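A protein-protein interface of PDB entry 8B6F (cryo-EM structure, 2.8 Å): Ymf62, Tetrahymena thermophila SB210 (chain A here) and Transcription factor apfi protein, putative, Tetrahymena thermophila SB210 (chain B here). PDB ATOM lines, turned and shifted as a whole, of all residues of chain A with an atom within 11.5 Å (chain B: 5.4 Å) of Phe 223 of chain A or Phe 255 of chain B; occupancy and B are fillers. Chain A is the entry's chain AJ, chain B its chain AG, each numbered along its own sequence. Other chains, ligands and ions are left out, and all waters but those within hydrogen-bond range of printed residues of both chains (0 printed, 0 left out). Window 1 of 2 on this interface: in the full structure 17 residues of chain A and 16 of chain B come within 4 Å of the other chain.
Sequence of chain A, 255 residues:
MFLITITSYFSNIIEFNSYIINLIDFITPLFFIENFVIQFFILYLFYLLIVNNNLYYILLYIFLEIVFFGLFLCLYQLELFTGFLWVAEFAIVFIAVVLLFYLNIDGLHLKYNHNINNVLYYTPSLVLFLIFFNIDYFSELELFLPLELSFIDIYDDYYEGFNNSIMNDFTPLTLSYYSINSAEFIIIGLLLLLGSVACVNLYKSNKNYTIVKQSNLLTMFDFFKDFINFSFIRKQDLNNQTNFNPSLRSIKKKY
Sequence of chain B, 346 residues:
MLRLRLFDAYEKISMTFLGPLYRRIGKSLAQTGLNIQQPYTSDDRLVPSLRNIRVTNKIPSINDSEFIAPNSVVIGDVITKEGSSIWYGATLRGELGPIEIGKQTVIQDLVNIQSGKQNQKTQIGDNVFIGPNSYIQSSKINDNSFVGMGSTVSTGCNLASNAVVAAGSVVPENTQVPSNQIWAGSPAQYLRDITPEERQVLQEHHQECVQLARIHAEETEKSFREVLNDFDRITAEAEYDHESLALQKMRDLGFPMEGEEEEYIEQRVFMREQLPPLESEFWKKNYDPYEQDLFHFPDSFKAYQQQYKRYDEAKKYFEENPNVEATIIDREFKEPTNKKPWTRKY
The side-chain carboxylate (OD2) of Asp 226 of chain A is in hydrogen-bond range of the backbone NH (N) of Asp 222 of chain A, 3.0 Å away.
The backbone carbonyl oxygen (O) of Met 250 of chain B lies within hydrogen-bond range of the backbone NH (N) of Phe 255 of chain B (2.9 Å).
The guanidinium group (NH2) of Arg 272 of chain B lies within hydrogen-bond range of the backbone carbonyl oxygen (O) of Leu 253 of chain B, 3.4 Å away.
The guanidinium group (NH2) of Arg 272 of chain B sits at hydrogen-bond distance from the backbone carbonyl oxygen (O) of Arg 268 of chain B.
Leu 218 of chain A touches Leu 253 of chain B.
CB of Phe 223 of chain A touches CD2 of Leu 253 of chain B, at 3.5 Å.
Phe 223 of chain A touches Phe 255 of chain B.
Phe 223 of chain A touches Val 269 of chain B (CZ to O, 3.0 Å).
Phe 224 of chain A touches Arg 272 of chain B (CZ to NH1, 3.3 Å).
Phe 224 of chain A touches Gln 274 of chain B.
Asp 226 of chain A touches Gln 274 of chain B (O to NE2, 3.6 Å).
Phe 227 of chain A touches Gln 274 of chain B.
Val 269 of chain B touches Phe 230 of chain A.
Phe 270 of chain B touches Phe 232 of chain A (CB to CZ, 3.7 Å).
Of the printed residues of chain B, Phe 223 of chain A touches Leu 253 (3.5 Å), Phe 255 (3.7 Å) and Val 269 (3.0 Å).
Phe 255 of chain B touches just one residue of chain A: Phe 223.
Of chain A, only Gln 214 (3.1 Å) comes within 4 Å of Met 250 of chain B.
Of chain A, only Leu 218 (3.9 Å) and Phe 223 (3.5 Å) come within 4 Å of Leu 253 of chain B.
Of chain A, only Phe 223 and Phe 230 come within 4 Å of Val 269 of chain B.
Arg 272 of chain B touches just one residue of chain A: Phe 224.
Of the printed residues of chain B, Phe 227 of chain A touches Gln 274.
Printed residues of chain B within 4 Å of Asp 226 of chain A: Gln 274 (3.6 Å).
Printed residues of chain B within 4 Å of Leu 218 of chain A: Leu 253 (3.9 Å).
Of the printed residues of chain B, Phe 232 of chain A touches Phe 270 (3.7 Å).
Ser 231 of chain A touches none of the printed residues of chain B.
Arg 268 of chain B touches none of the printed residues of chain A.
The nearest printed residue of chain B that does not touch Phe 223 of chain A is Arg 268 of chain B (4.01 Å).
Of the 22 printed residues of chain A, 8 touch a printed residue of chain B.
Among the printed residues, 11 pairs touch across the chains.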
ATOM      1  N   ILE A 211     -22.381 -12.437   8.893  1.00  0.00           N
ATOM      2  CA  ILE A 211     -23.322 -11.768   9.787  1.00  0.00           C
ATOM      3  C   ILE A 211     -24.183 -12.754  10.566  1.00  0.00           C
ATOM      4  O   ILE A 211     -24.749 -12.382  11.600  1.00  0.00           O
ATOM      5  CB  ILE A 211     -24.231 -10.813   8.992  1.00  0.00           C
ATOM      6  CG1 ILE A 211     -23.393  -9.790   8.219  1.00  0.00           C
ATOM      7  CG2 ILE A 211     -25.213 -10.101   9.917  1.00  0.00           C
ATOM      8  CD1 ILE A 211     -24.197  -8.932   7.257  1.00  0.00           C
ATOM      9  N   LYS A 213     -23.789 -15.252  12.641  1.00  0.00           N
ATOM     10  CA  LYS A 213     -23.512 -15.609  14.027  1.00  0.00           C
ATOM     11  C   LYS A 213     -23.120 -14.423  14.898  1.00  0.00           C
ATOM     12  O   LYS A 213     -22.849 -14.614  16.086  1.00  0.00           O
ATOM     13  CB  LYS A 213     -22.408 -16.667  14.082  1.00  0.00           C
ATOM     14  CG  LYS A 213     -22.851 -18.028  13.571  1.00  0.00           C
ATOM     15  CD  LYS A 213     -21.805 -19.091  13.832  1.00  0.00           C
ATOM     16  CE  LYS A 213     -22.315 -20.465  13.434  1.00  0.00           C
ATOM     17  NZ  LYS A 213     -21.304 -21.529  13.689  1.00  0.00           N
ATOM     18  N   GLN A 214     -23.080 -13.209  14.348  1.00  0.00           N
ATOM     19  CA  GLN A 214     -22.670 -12.060  15.151  1.00  0.00           C
ATOM     20  C   GLN A 214     -23.656 -11.796  16.281  1.00  0.00           C
ATOM     21  O   GLN A 214     -23.260 -11.404  17.383  1.00  0.00           O
ATOM     22  CB  GLN A 214     -22.527 -10.824  14.265  1.00  0.00           C
ATOM     23  CG  GLN A 214     -21.552 -11.010  13.124  1.00  0.00           C
ATOM     24  CD  GLN A 214     -21.309  -9.729  12.360  1.00  0.00           C
ATOM     25  OE1 GLN A 214     -21.752  -8.658  12.768  1.00  0.00           O
ATOM     26  NE2 GLN A 214     -20.601  -9.832  11.241  1.00  0.00           N
ATOM     27  N   SER A 215     -24.949 -12.004  16.025  1.00  0.00           N
ATOM     28  CA  SER A 215     -25.956 -11.785  17.058  1.00  0.00           C
ATOM     29  C   SER A 215     -25.695 -12.658  18.277  1.00  0.00           C
ATOM     30  O   SER A 215     -25.657 -12.167  19.411  1.00  0.00           O
ATOM     31  CB  SER A 215     -27.349 -12.062  16.493  1.00  0.00           C
ATOM     32  OG  SER A 215     -28.331 -11.971  17.510  1.00  0.00           O
ATOM     33  N   ASN A 216     -25.519 -13.962  18.065  1.00  0.00           N
ATOM     34  CA  ASN A 216     -25.261 -14.857  19.187  1.00  0.00           C
ATOM     35  C   ASN A 216     -23.927 -14.541  19.850  1.00  0.00           C
ATOM     36  O   ASN A 216     -23.808 -14.609  21.077  1.00  0.00           O
ATOM     37  CB  ASN A 216     -25.296 -16.311  18.723  1.00  0.00           C
ATOM     38  CG  ASN A 216     -25.154 -17.287  19.873  1.00  0.00           C
ATOM     39  OD1 ASN A 216     -24.053 -17.737  20.189  1.00  0.00           O
ATOM     40  ND2 ASN A 216     -26.270 -17.608  20.514  1.00  0.00           N
ATOM     41  N   LEU A 217     -22.910 -14.207  19.055  1.00  0.00           N
ATOM     42  CA  LEU A 217     -21.618 -13.845  19.627  1.00  0.00           C
ATOM     43  C   LEU A 217     -21.766 -12.690  20.608  1.00  0.00           C
ATOM     44  O   LEU A 217     -21.305 -12.767  21.752  1.00  0.00           O
ATOM     45  CB  LEU A 217     -20.637 -13.480  18.512  1.00  0.00           C
ATOM     46  CG  LEU A 217     -19.237 -13.046  18.954  1.00  0.00           C
ATOM     47  CD1 LEU A 217     -18.495 -14.200  19.600  1.00  0.00           C
ATOM     48  CD2 LEU A 217     -18.452 -12.498  17.778  1.00  0.00           C
ATOM     49  N   LEU A 218     -22.405 -11.605  20.174  1.00  0.00           N
ATOM     50  CA  LEU A 218     -22.544 -10.435  21.033  1.00  0.00           C
ATOM     51  C   LEU A 218     -23.507 -10.689  22.184  1.00  0.00           C
ATOM     52  O   LEU A 218     -23.402 -10.042  23.231  1.00  0.00           O
ATOM     53  CB  LEU A 218     -23.004  -9.232  20.211  1.00  0.00           C
ATOM     54  CG  LEU A 218     -22.049  -8.782  19.101  1.00  0.00           C
ATOM     55  CD1 LEU A 218     -22.673  -7.671  18.279  1.00  0.00           C
ATOM     56  CD2 LEU A 218     -20.715  -8.333  19.677  1.00  0.00           C
ATOM     57  N   THR A 219     -24.450 -11.617  22.014  1.00  0.00           N
ATOM     58  CA  THR A 219     -25.397 -11.908  23.084  1.00  0.00           C
ATOM     59  C   THR A 219     -24.745 -12.703  24.208  1.00  0.00           C
ATOM     60  O   THR A 219     -24.989 -12.431  25.389  1.00  0.00           O
ATOM     61  CB  THR A 219     -26.594 -12.676  22.524  1.00  0.00           C
ATOM     62  OG1 THR A 219     -27.187 -11.933  21.453  1.00  0.00           O
ATOM     63  CG2 THR A 219     -27.640 -12.919  23.603  1.00  0.00           C
ATOM     64  N   MET A 220     -23.915 -13.688  23.865  1.00  0.00           N
ATOM     65  CA  MET A 220     -23.364 -14.599  24.858  1.00  0.00           C
ATOM     66  C   MET A 220     -21.986 -14.201  25.367  1.00  0.00           C
ATOM     67  O   MET A 220     -21.575 -14.689  26.424  1.00  0.00           O
ATOM     68  CB  MET A 220     -23.285 -16.018  24.282  1.00  0.00           C
ATOM     69  CG  MET A 220     -24.623 -16.582  23.827  1.00  0.00           C
ATOM     70  SD  MET A 220     -25.894 -16.550  25.107  1.00  0.00           S
ATOM     71  CE  MET A 220     -25.124 -17.533  26.386  1.00  0.00           C
ATOM     72  N   PHE A 221     -21.264 -13.341  24.653  1.00  0.00           N
ATOM     73  CA  PHE A 221     -19.936 -12.905  25.062  1.00  0.00           C
ATOM     74  C   PHE A 221     -19.945 -11.407  25.323  1.00  0.00           C
ATOM     75  O   PHE A 221     -20.461 -10.634  24.509  1.00  0.00           O
ATOM     76  CB  PHE A 221     -18.895 -13.250  23.994  1.00  0.00           C
ATOM     77  CG  PHE A 221     -18.654 -14.723  23.842  1.00  0.00           C
ATOM     78  CD1 PHE A 221     -17.684 -15.359  24.597  1.00  0.00           C
ATOM     79  CD2 PHE A 221     -19.402 -15.470  22.949  1.00  0.00           C
ATOM     80  CE1 PHE A 221     -17.464 -16.716  24.462  1.00  0.00           C
ATOM     81  CE2 PHE A 221     -19.188 -16.827  22.809  1.00  0.00           C
ATOM     82  CZ  PHE A 221     -18.216 -17.452  23.567  1.00  0.00           C
ATOM     83  N   ASP A 222     -19.378 -11.004  26.456  1.00  0.00           N
ATOM     84  CA  ASP A 222     -19.287  -9.590  26.788  1.00  0.00           C
ATOM     85  C   ASP A 222     -18.282  -8.905  25.871  1.00  0.00           C
ATOM     86  O   ASP A 222     -17.139  -9.349  25.744  1.00  0.00           O
ATOM     87  CB  ASP A 222     -18.874  -9.413  28.247  1.00  0.00           C
ATOM     88  CG  ASP A 222     -19.820 -10.104  29.206  1.00  0.00           C
ATOM     89  OD1 ASP A 222     -21.022 -10.213  28.885  1.00  0.00           O
ATOM     90  OD2 ASP A 222     -19.360 -10.544  30.281  1.00  0.00           O
ATOM     91  N   PHE A 223     -18.709  -7.816  25.232  1.00  0.00           N
ATOM     92  CA  PHE A 223     -17.835  -7.131  24.291  1.00  0.00           C
ATOM     93  C   PHE A 223     -16.672  -6.435  24.984  1.00  0.00           C
ATOM     94  O   PHE A 223     -15.659  -6.157  24.335  1.00  0.00           O
ATOM     95  CB  PHE A 223     -18.634  -6.116  23.475  1.00  0.00           C
ATOM     96  CG  PHE A 223     -17.843  -5.470  22.379  1.00  0.00           C
ATOM     97  CD1 PHE A 223     -17.446  -6.203  21.275  1.00  0.00           C
ATOM     98  CD2 PHE A 223     -17.501  -4.132  22.447  1.00  0.00           C
ATOM     99  CE1 PHE A 223     -16.718  -5.616  20.261  1.00  0.00           C
ATOM    100  CE2 PHE A 223     -16.774  -3.536  21.435  1.00  0.00           C
ATOM    101  CZ  PHE A 223     -16.382  -4.280  20.340  1.00  0.00           C
ATOM    102  N   PHE A 224     -16.786  -6.159  26.280  1.00  0.00           N
ATOM    103  CA  PHE A 224     -15.754  -5.456  27.031  1.00  0.00           C
ATOM    104  C   PHE A 224     -14.978  -6.354  27.978  1.00  0.00           C
ATOM    105  O   PHE A 224     -13.755  -6.236  28.065  1.00  0.00           O
ATOM    106  CB  PHE A 224     -16.378  -4.304  27.828  1.00  0.00           C
ATOM    107  CG  PHE A 224     -17.300  -3.443  27.017  1.00  0.00           C
ATOM    108  CD1 PHE A 224     -16.802  -2.606  26.032  1.00  0.00           C
ATOM    109  CD2 PHE A 224     -18.667  -3.467  27.242  1.00  0.00           C
ATOM    110  CE1 PHE A 224     -17.649  -1.813  25.283  1.00  0.00           C
ATOM    111  CE2 PHE A 224     -19.520  -2.677  26.497  1.00  0.00           C
ATOM    112  CZ  PHE A 224     -19.009  -1.847  25.516  1.00  0.00           C
ATOM    113  N   LYS A 225     -15.654  -7.244  28.705  1.00  0.00           N
ATOM    114  CA  LYS A 225     -14.948  -8.118  29.634  1.00  0.00           C
ATOM    115  C   LYS A 225     -14.200  -9.224  28.900  1.00  0.00           C
ATOM    116  O   LYS A 225     -13.056  -9.539  29.245  1.00  0.00           O
ATOM    117  CB  LYS A 225     -15.929  -8.713  30.643  1.00  0.00           C
ATOM    118  CG  LYS A 225     -16.584  -7.673  31.539  1.00  0.00           C
ATOM    119  CD  LYS A 225     -16.605  -8.115  32.996  1.00  0.00           C
ATOM    120  CE  LYS A 225     -15.214  -8.062  33.619  1.00  0.00           C
ATOM    121  NZ  LYS A 225     -15.230  -8.428  35.064  1.00  0.00           N
ATOM    122  N   ASP A 226     -14.822  -9.824  27.890  1.00  0.00           N
ATOM    123  CA  ASP A 226     -14.220 -10.934  27.165  1.00  0.00           C
ATOM    124  C   ASP A 226     -13.380 -10.420  26.004  1.00  0.00           C
ATOM    125  O   ASP A 226     -13.761  -9.469  25.316  1.00  0.00           O
ATOM    126  CB  ASP A 226     -15.295 -11.890  26.645  1.00  0.00           C
ATOM    127  CG  ASP A 226     -16.068 -12.558  27.764  1.00  0.00           C
ATOM    128  OD1 ASP A 226     -15.465 -12.850  28.816  1.00  0.00           O
ATOM    129  OD2 ASP A 226     -17.282 -12.792  27.592  1.00  0.00           O
ATOM    130  N   PHE A 227     -12.234 -11.063  25.790  1.00  0.00           N
ATOM    131  CA  PHE A 227     -11.290 -10.664  24.748  1.00  0.00           C
ATOM    132  C   PHE A 227     -11.612 -11.468  23.496  1.00  0.00           C
ATOM    133  O   PHE A 227     -11.153 -12.595  23.317  1.00  0.00           O
ATOM    134  CB  PHE A 227      -9.856 -10.885  25.219  1.00  0.00           C
ATOM    135  CG  PHE A 227      -8.816 -10.366  24.272  1.00  0.00           C
ATOM    136  CD1 PHE A 227      -8.759  -9.020  23.955  1.00  0.00           C
ATOM    137  CD2 PHE A 227      -7.875 -11.219  23.724  1.00  0.00           C
ATOM    138  CE1 PHE A 227      -7.795  -8.537  23.093  1.00  0.00           C
ATOM    139  CE2 PHE A 227      -6.908 -10.743  22.860  1.00  0.00           C
ATOM    140  CZ  PHE A 227      -6.867  -9.400  22.545  1.00  0.00           C
ATOM    141  N   ILE A 228     -12.413 -10.875  22.613  1.00  0.00           N
ATOM    142  CA  ILE A 228     -12.870 -11.520  21.388  1.00  0.00           C
ATOM    143  C   ILE A 228     -12.116 -10.915  20.214  1.00  0.00           C
ATOM    144  O   ILE A 228     -11.996  -9.689  20.108  1.00  0.00           O
ATOM    145  CB  ILE A 228     -14.391 -11.376  21.201  1.00  0.00           C
ATOM    146  CG1 ILE A 228     -14.783  -9.897  21.107  1.00  0.00           C
ATOM    147  CG2 ILE A 228     -15.121 -12.074  22.343  1.00  0.00           C
ATOM    148  CD1 ILE A 228     -16.274  -9.651  21.001  1.00  0.00           C
ATOM    149  N   ASN A 229     -11.601 -11.774  19.340  1.00  0.00           N
ATOM    150  CA  ASN A 229     -10.869 -11.319  18.170  1.00  0.00           C
ATOM    151  C   ASN A 229     -11.828 -10.811  17.104  1.00  0.00           C
ATOM    152  O   ASN A 229     -12.887 -11.399  16.868  1.00  0.00           O
ATOM    153  CB  ASN A 229     -10.017 -12.456  17.604  1.00  0.00           C
ATOM    154  CG  ASN A 229      -9.236 -12.039  16.378  1.00  0.00           C
ATOM    155  OD1 ASN A 229      -8.947 -10.860  16.183  1.00  0.00           O
ATOM    156  ND2 ASN A 229      -8.889 -13.008  15.540  1.00  0.00           N
ATOM    157  N   PHE A 230     -11.454  -9.709  16.462  1.00  0.00           N
ATOM    158  CA  PHE A 230     -12.239  -9.167  15.364  1.00  0.00           C
ATOM    159  C   PHE A 230     -11.346  -8.266  14.526  1.00  0.00           C
ATOM    160  O   PHE A 230     -10.277  -7.838  14.965  1.00  0.00           O
ATOM    161  CB  PHE A 230     -13.465  -8.397  15.868  1.00  0.00           C
ATOM    162  CG  PHE A 230     -13.125  -7.168  16.659  1.00  0.00           C
ATOM    163  CD1 PHE A 230     -12.907  -7.246  18.024  1.00  0.00           C
ATOM    164  CD2 PHE A 230     -13.038  -5.933  16.041  1.00  0.00           C
ATOM    165  CE1 PHE A 230     -12.597  -6.118  18.755  1.00  0.00           C
ATOM    166  CE2 PHE A 230     -12.730  -4.801  16.764  1.00  0.00           C
ATOM    167  CZ  PHE A 230     -12.510  -4.893  18.123  1.00  0.00           C
ATOM    168  N   SER A 231     -11.802  -7.991  13.308  1.00  0.00           N
ATOM    169  CA  SER A 231     -11.113  -7.099  12.391  1.00  0.00           C
ATOM    170  C   SER A 231     -12.091  -6.039  11.907  1.00  0.00           C
ATOM    171  O   SER A 231     -13.291  -6.294  11.784  1.00  0.00           O
ATOM    172  CB  SER A 231     -10.530  -7.867  11.200  1.00  0.00           C
ATOM    173  OG  SER A 231      -9.855  -6.998  10.308  1.00  0.00           O
ATOM    174  N   PHE A 232     -11.570  -4.845  11.634  1.00  0.00           N
ATOM    175  CA  PHE A 232     -12.419  -3.743  11.211  1.00  0.00           C
ATOM    176  C   PHE A 232     -11.624  -2.797  10.325  1.00  0.00           C
ATOM    177  O   PHE A 232     -10.392  -2.805  10.317  1.00  0.00           O
ATOM    178  CB  PHE A 232     -13.001  -2.987  12.412  1.00  0.00           C
ATOM    179  CG  PHE A 232     -11.971  -2.271  13.232  1.00  0.00           C
ATOM    180  CD1 PHE A 232     -11.225  -2.950  14.180  1.00  0.00           C
ATOM    181  CD2 PHE A 232     -11.755  -0.915  13.061  1.00  0.00           C
ATOM    182  CE1 PHE A 232     -10.277  -2.292  14.935  1.00  0.00           C
ATOM    183  CE2 PHE A 232     -10.809  -0.250  13.814  1.00  0.00           C
ATOM    184  CZ  PHE A 232     -10.069  -0.940  14.752  1.00  0.00           C
ATOM    185  N   ILE A 233     -12.358  -1.981   9.570  1.00  0.00           N
ATOM    186  CA  ILE A 233     -11.789  -0.979   8.680  1.00  0.00           C
ATOM    187  C   ILE A 233     -12.355   0.379   9.069  1.00  0.00           C
ATOM    188  O   ILE A 233     -13.554   0.507   9.339  1.00  0.00           O
ATOM    189  CB  ILE A 233     -12.091  -1.293   7.200  1.00  0.00           C
ATOM    190  CG1 ILE A 233     -11.549  -2.678   6.843  1.00  0.00           C
ATOM    191  CG2 ILE A 233     -11.490  -0.224   6.291  1.00  0.00           C
ATOM    192  CD1 ILE A 233     -11.869  -3.126   5.434  1.00  0.00           C
ATOM    193  N   MET B 250     -25.856  -4.537  18.296  1.00  0.00           N
ATOM    194  CA  MET B 250     -24.875  -3.481  18.061  1.00  0.00           C
ATOM    195  C   MET B 250     -25.349  -2.140  18.605  1.00  0.00           C
ATOM    196  O   MET B 250     -24.568  -1.404  19.218  1.00  0.00           O
ATOM    197  CB  MET B 250     -24.577  -3.367  16.567  1.00  0.00           C
ATOM    198  CG  MET B 250     -23.762  -4.518  16.010  1.00  0.00           C
ATOM    199  SD  MET B 250     -23.545  -4.397  14.230  1.00  0.00           S
ATOM    200  CE  MET B 250     -22.751  -5.962  13.900  1.00  0.00           C
ATOM    201  N   ARG B 251     -26.620  -1.797  18.392  1.00  0.00           N
ATOM    202  CA  ARG B 251     -27.120  -0.530  18.917  1.00  0.00           C
ATOM    203  C   ARG B 251     -27.164  -0.549  20.439  1.00  0.00           C
ATOM    204  O   ARG B 251     -26.919   0.477  21.083  1.00  0.00           O
ATOM    205  CB  ARG B 251     -28.499  -0.216  18.333  1.00  0.00           C
ATOM    206  CG  ARG B 251     -29.615  -1.135  18.801  1.00  0.00           C
ATOM    207  CD  ARG B 251     -30.980  -0.594  18.414  1.00  0.00           C
ATOM    208  NE  ARG B 251     -32.052  -1.461  18.885  1.00  0.00           N
ATOM    209  CZ  ARG B 251     -32.537  -1.459  20.118  1.00  0.00           C
ATOM    210  NH1 ARG B 251     -32.066  -0.641  21.045  1.00  0.00           N
ATOM    211  NH2 ARG B 251     -33.518  -2.301  20.430  1.00  0.00           N
ATOM    212  N   LEU B 253     -25.008  -2.143  22.289  1.00  0.00           N
ATOM    213  CA  LEU B 253     -23.620  -1.949  22.692  1.00  0.00           C
ATOM    214  C   LEU B 253     -23.157  -0.519  22.446  1.00  0.00           C
ATOM    215  O   LEU B 253     -22.253  -0.037  23.138  1.00  0.00           O
ATOM    216  CB  LEU B 253     -22.714  -2.932  21.952  1.00  0.00           C
ATOM    217  CG  LEU B 253     -22.458  -4.269  22.651  1.00  0.00           C
ATOM    218  CD1 LEU B 253     -23.749  -5.007  22.972  1.00  0.00           C
ATOM    219  CD2 LEU B 253     -21.556  -5.134  21.788  1.00  0.00           C
ATOM    220  N   GLY B 254     -23.745   0.162  21.475  1.00  0.00           N
ATOM    221  CA  GLY B 254     -23.405   1.530  21.168  1.00  0.00           C
ATOM    222  C   GLY B 254     -22.653   1.754  19.869  1.00  0.00           C
ATOM    223  O   GLY B 254     -21.993   2.791  19.735  1.00  0.00           O
ATOM    224  N   PHE B 255     -22.726   0.828  18.917  1.00  0.00           N
ATOM    225  CA  PHE B 255     -22.031   1.007  17.655  1.00  0.00           C
ATOM    226  C   PHE B 255     -22.712   2.089  16.820  1.00  0.00           C
ATOM    227  O   PHE B 255     -23.881   2.414  17.040  1.00  0.00           O
ATOM    228  CB  PHE B 255     -22.000  -0.301  16.867  1.00  0.00           C
ATOM    229  CG  PHE B 255     -21.123  -1.366  17.471  1.00  0.00           C
ATOM    230  CD1 PHE B 255     -20.553  -1.205  18.725  1.00  0.00           C
ATOM    231  CD2 PHE B 255     -20.856  -2.527  16.767  1.00  0.00           C
ATOM    232  CE1 PHE B 255     -19.748  -2.187  19.266  1.00  0.00           C
ATOM    233  CE2 PHE B 255     -20.053  -3.512  17.302  1.00  0.00           C
ATOM    234  CZ  PHE B 255     -19.497  -3.342  18.553  1.00  0.00           C
ATOM    235  N   PRO B 256     -21.995   2.672  15.860  1.00  0.00           N
ATOM    236  CA  PRO B 256     -22.635   3.641  14.962  1.00  0.00           C
ATOM    237  C   PRO B 256     -23.771   2.996  14.185  1.00  0.00           C
ATOM    238  O   PRO B 256     -23.672   1.848  13.748  1.00  0.00           O
ATOM    239  CB  PRO B 256     -21.494   4.077  14.034  1.00  0.00           C
ATOM    240  CG  PRO B 256     -20.243   3.716  14.755  1.00  0.00           C
ATOM    241  CD  PRO B 256     -20.566   2.498  15.555  1.00  0.00           C
ATOM    242  N   MET B 257     -24.852   3.756  13.997  1.00  0.00           N
ATOM    243  CA  MET B 257     -26.032   3.275  13.285  1.00  0.00           C
ATOM    244  C   MET B 257     -26.391   4.164  12.098  1.00  0.00           C
ATOM    245  O   MET B 257     -27.504   4.068  11.572  1.00  0.00           O
ATOM    246  CB  MET B 257     -27.221   3.173  14.242  1.00  0.00           C
ATOM    247  CG  MET B 257     -27.041   2.162  15.370  1.00  0.00           C
ATOM    248  SD  MET B 257     -27.354   0.447  14.894  1.00  0.00           S
ATOM    249  CE  MET B 257     -25.736  -0.112  14.374  1.00  0.00           C
ATOM    250  N   ARG B 268     -15.883   3.326  19.241  1.00  0.00           N
ATOM    251  CA  ARG B 268     -16.918   2.565  19.923  1.00  0.00           C
ATOM    252  C   ARG B 268     -16.688   1.063  19.920  1.00  0.00           C
ATOM    253  O   ARG B 268     -17.337   0.362  20.703  1.00  0.00           O
ATOM    254  CB  ARG B 268     -18.290   2.844  19.288  1.00  0.00           C
ATOM    255  CG  ARG B 268     -19.005   4.054  19.865  1.00  0.00           C
ATOM    256  CD  ARG B 268     -19.457   3.801  21.295  1.00  0.00           C
ATOM    257  NE  ARG B 268     -20.486   4.742  21.716  1.00  0.00           N
ATOM    258  CZ  ARG B 268     -20.250   5.915  22.288  1.00  0.00           C
ATOM    259  NH1 ARG B 268     -19.018   6.333  22.529  1.00  0.00           N
ATOM    260  NH2 ARG B 268     -21.277   6.689  22.626  1.00  0.00           N
ATOM    261  N   VAL B 269     -15.792   0.552  19.081  1.00  0.00           N
ATOM    262  CA  VAL B 269     -15.562  -0.878  18.960  1.00  0.00           C
ATOM    263  C   VAL B 269     -14.197  -1.276  19.506  1.00  0.00           C
ATOM    264  O   VAL B 269     -14.065  -2.325  20.142  1.00  0.00           O
ATOM    265  CB  VAL B 269     -15.724  -1.337  17.492  1.00  0.00           C
ATOM    266  CG1 VAL B 269     -17.076  -0.910  16.947  1.00  0.00           C
ATOM    267  CG2 VAL B 269     -14.602  -0.797  16.615  1.00  0.00           C
ATOM    268  N   PHE B 270     -13.176  -0.455  19.281  1.00  0.00           N
ATOM    269  CA  PHE B 270     -11.801  -0.813  19.606  1.00  0.00           C
ATOM    270  C   PHE B 270     -11.162   0.095  20.642  1.00  0.00           C
ATOM    271  O   PHE B 270     -10.419  -0.390  21.499  1.00  0.00           O
ATOM    272  CB  PHE B 270     -10.953  -0.801  18.325  1.00  0.00           C
ATOM    273  CG  PHE B 270      -9.520  -1.183  18.545  1.00  0.00           C
ATOM    274  CD1 PHE B 270      -9.195  -2.368  19.182  1.00  0.00           C
ATOM    275  CD2 PHE B 270      -8.497  -0.368  18.094  1.00  0.00           C
ATOM    276  CE1 PHE B 270      -7.878  -2.725  19.380  1.00  0.00           C
ATOM    277  CE2 PHE B 270      -7.179  -0.719  18.290  1.00  0.00           C
ATOM    278  CZ  PHE B 270      -6.868  -1.898  18.933  1.00  0.00           C
ATOM    279  N   ARG B 272     -12.344   1.746  23.248  1.00  0.00           N
ATOM    280  CA  ARG B 272     -12.745   1.520  24.631  1.00  0.00           C
ATOM    281  C   ARG B 272     -11.944   0.376  25.237  1.00  0.00           C
ATOM    282  O   ARG B 272     -11.854  -0.713  24.663  1.00  0.00           O
ATOM    283  CB  ARG B 272     -14.241   1.218  24.711  1.00  0.00           C
ATOM    284  CG  ARG B 272     -15.116   2.451  24.578  1.00  0.00           C
ATOM    285  CD  ARG B 272     -16.577   2.138  24.854  1.00  0.00           C
ATOM    286  NE  ARG B 272     -17.195   1.395  23.763  1.00  0.00           N
ATOM    287  CZ  ARG B 272     -18.470   1.031  23.733  1.00  0.00           C
ATOM    288  NH1 ARG B 272     -19.295   1.314  24.727  1.00  0.00           N
ATOM    289  NH2 ARG B 272     -18.930   0.367  22.676  1.00  0.00           N
ATOM    290  N   GLN B 274     -10.821  -2.612  27.925  1.00  0.00           N
ATOM    291  CA  GLN B 274     -11.510  -3.733  28.543  1.00  0.00           C
ATOM    292  C   GLN B 274     -11.350  -3.681  30.054  1.00  0.00           C
ATOM    293  O   GLN B 274     -10.288  -3.318  30.568  1.00  0.00           O
ATOM    294  CB  GLN B 274     -10.970  -5.056  28.002  1.00  0.00           C
ATOM    295  CG  GLN B 274     -11.214  -5.227  26.518  1.00  0.00           C
ATOM    296  CD  GLN B 274     -10.875  -6.613  26.029  1.00  0.00           C
ATOM    297  OE1 GLN B 274     -10.246  -7.400  26.734  1.00  0.00           O
ATOM    298  NE2 GLN B 274     -11.299  -6.925  24.810  1.00  0.00           N
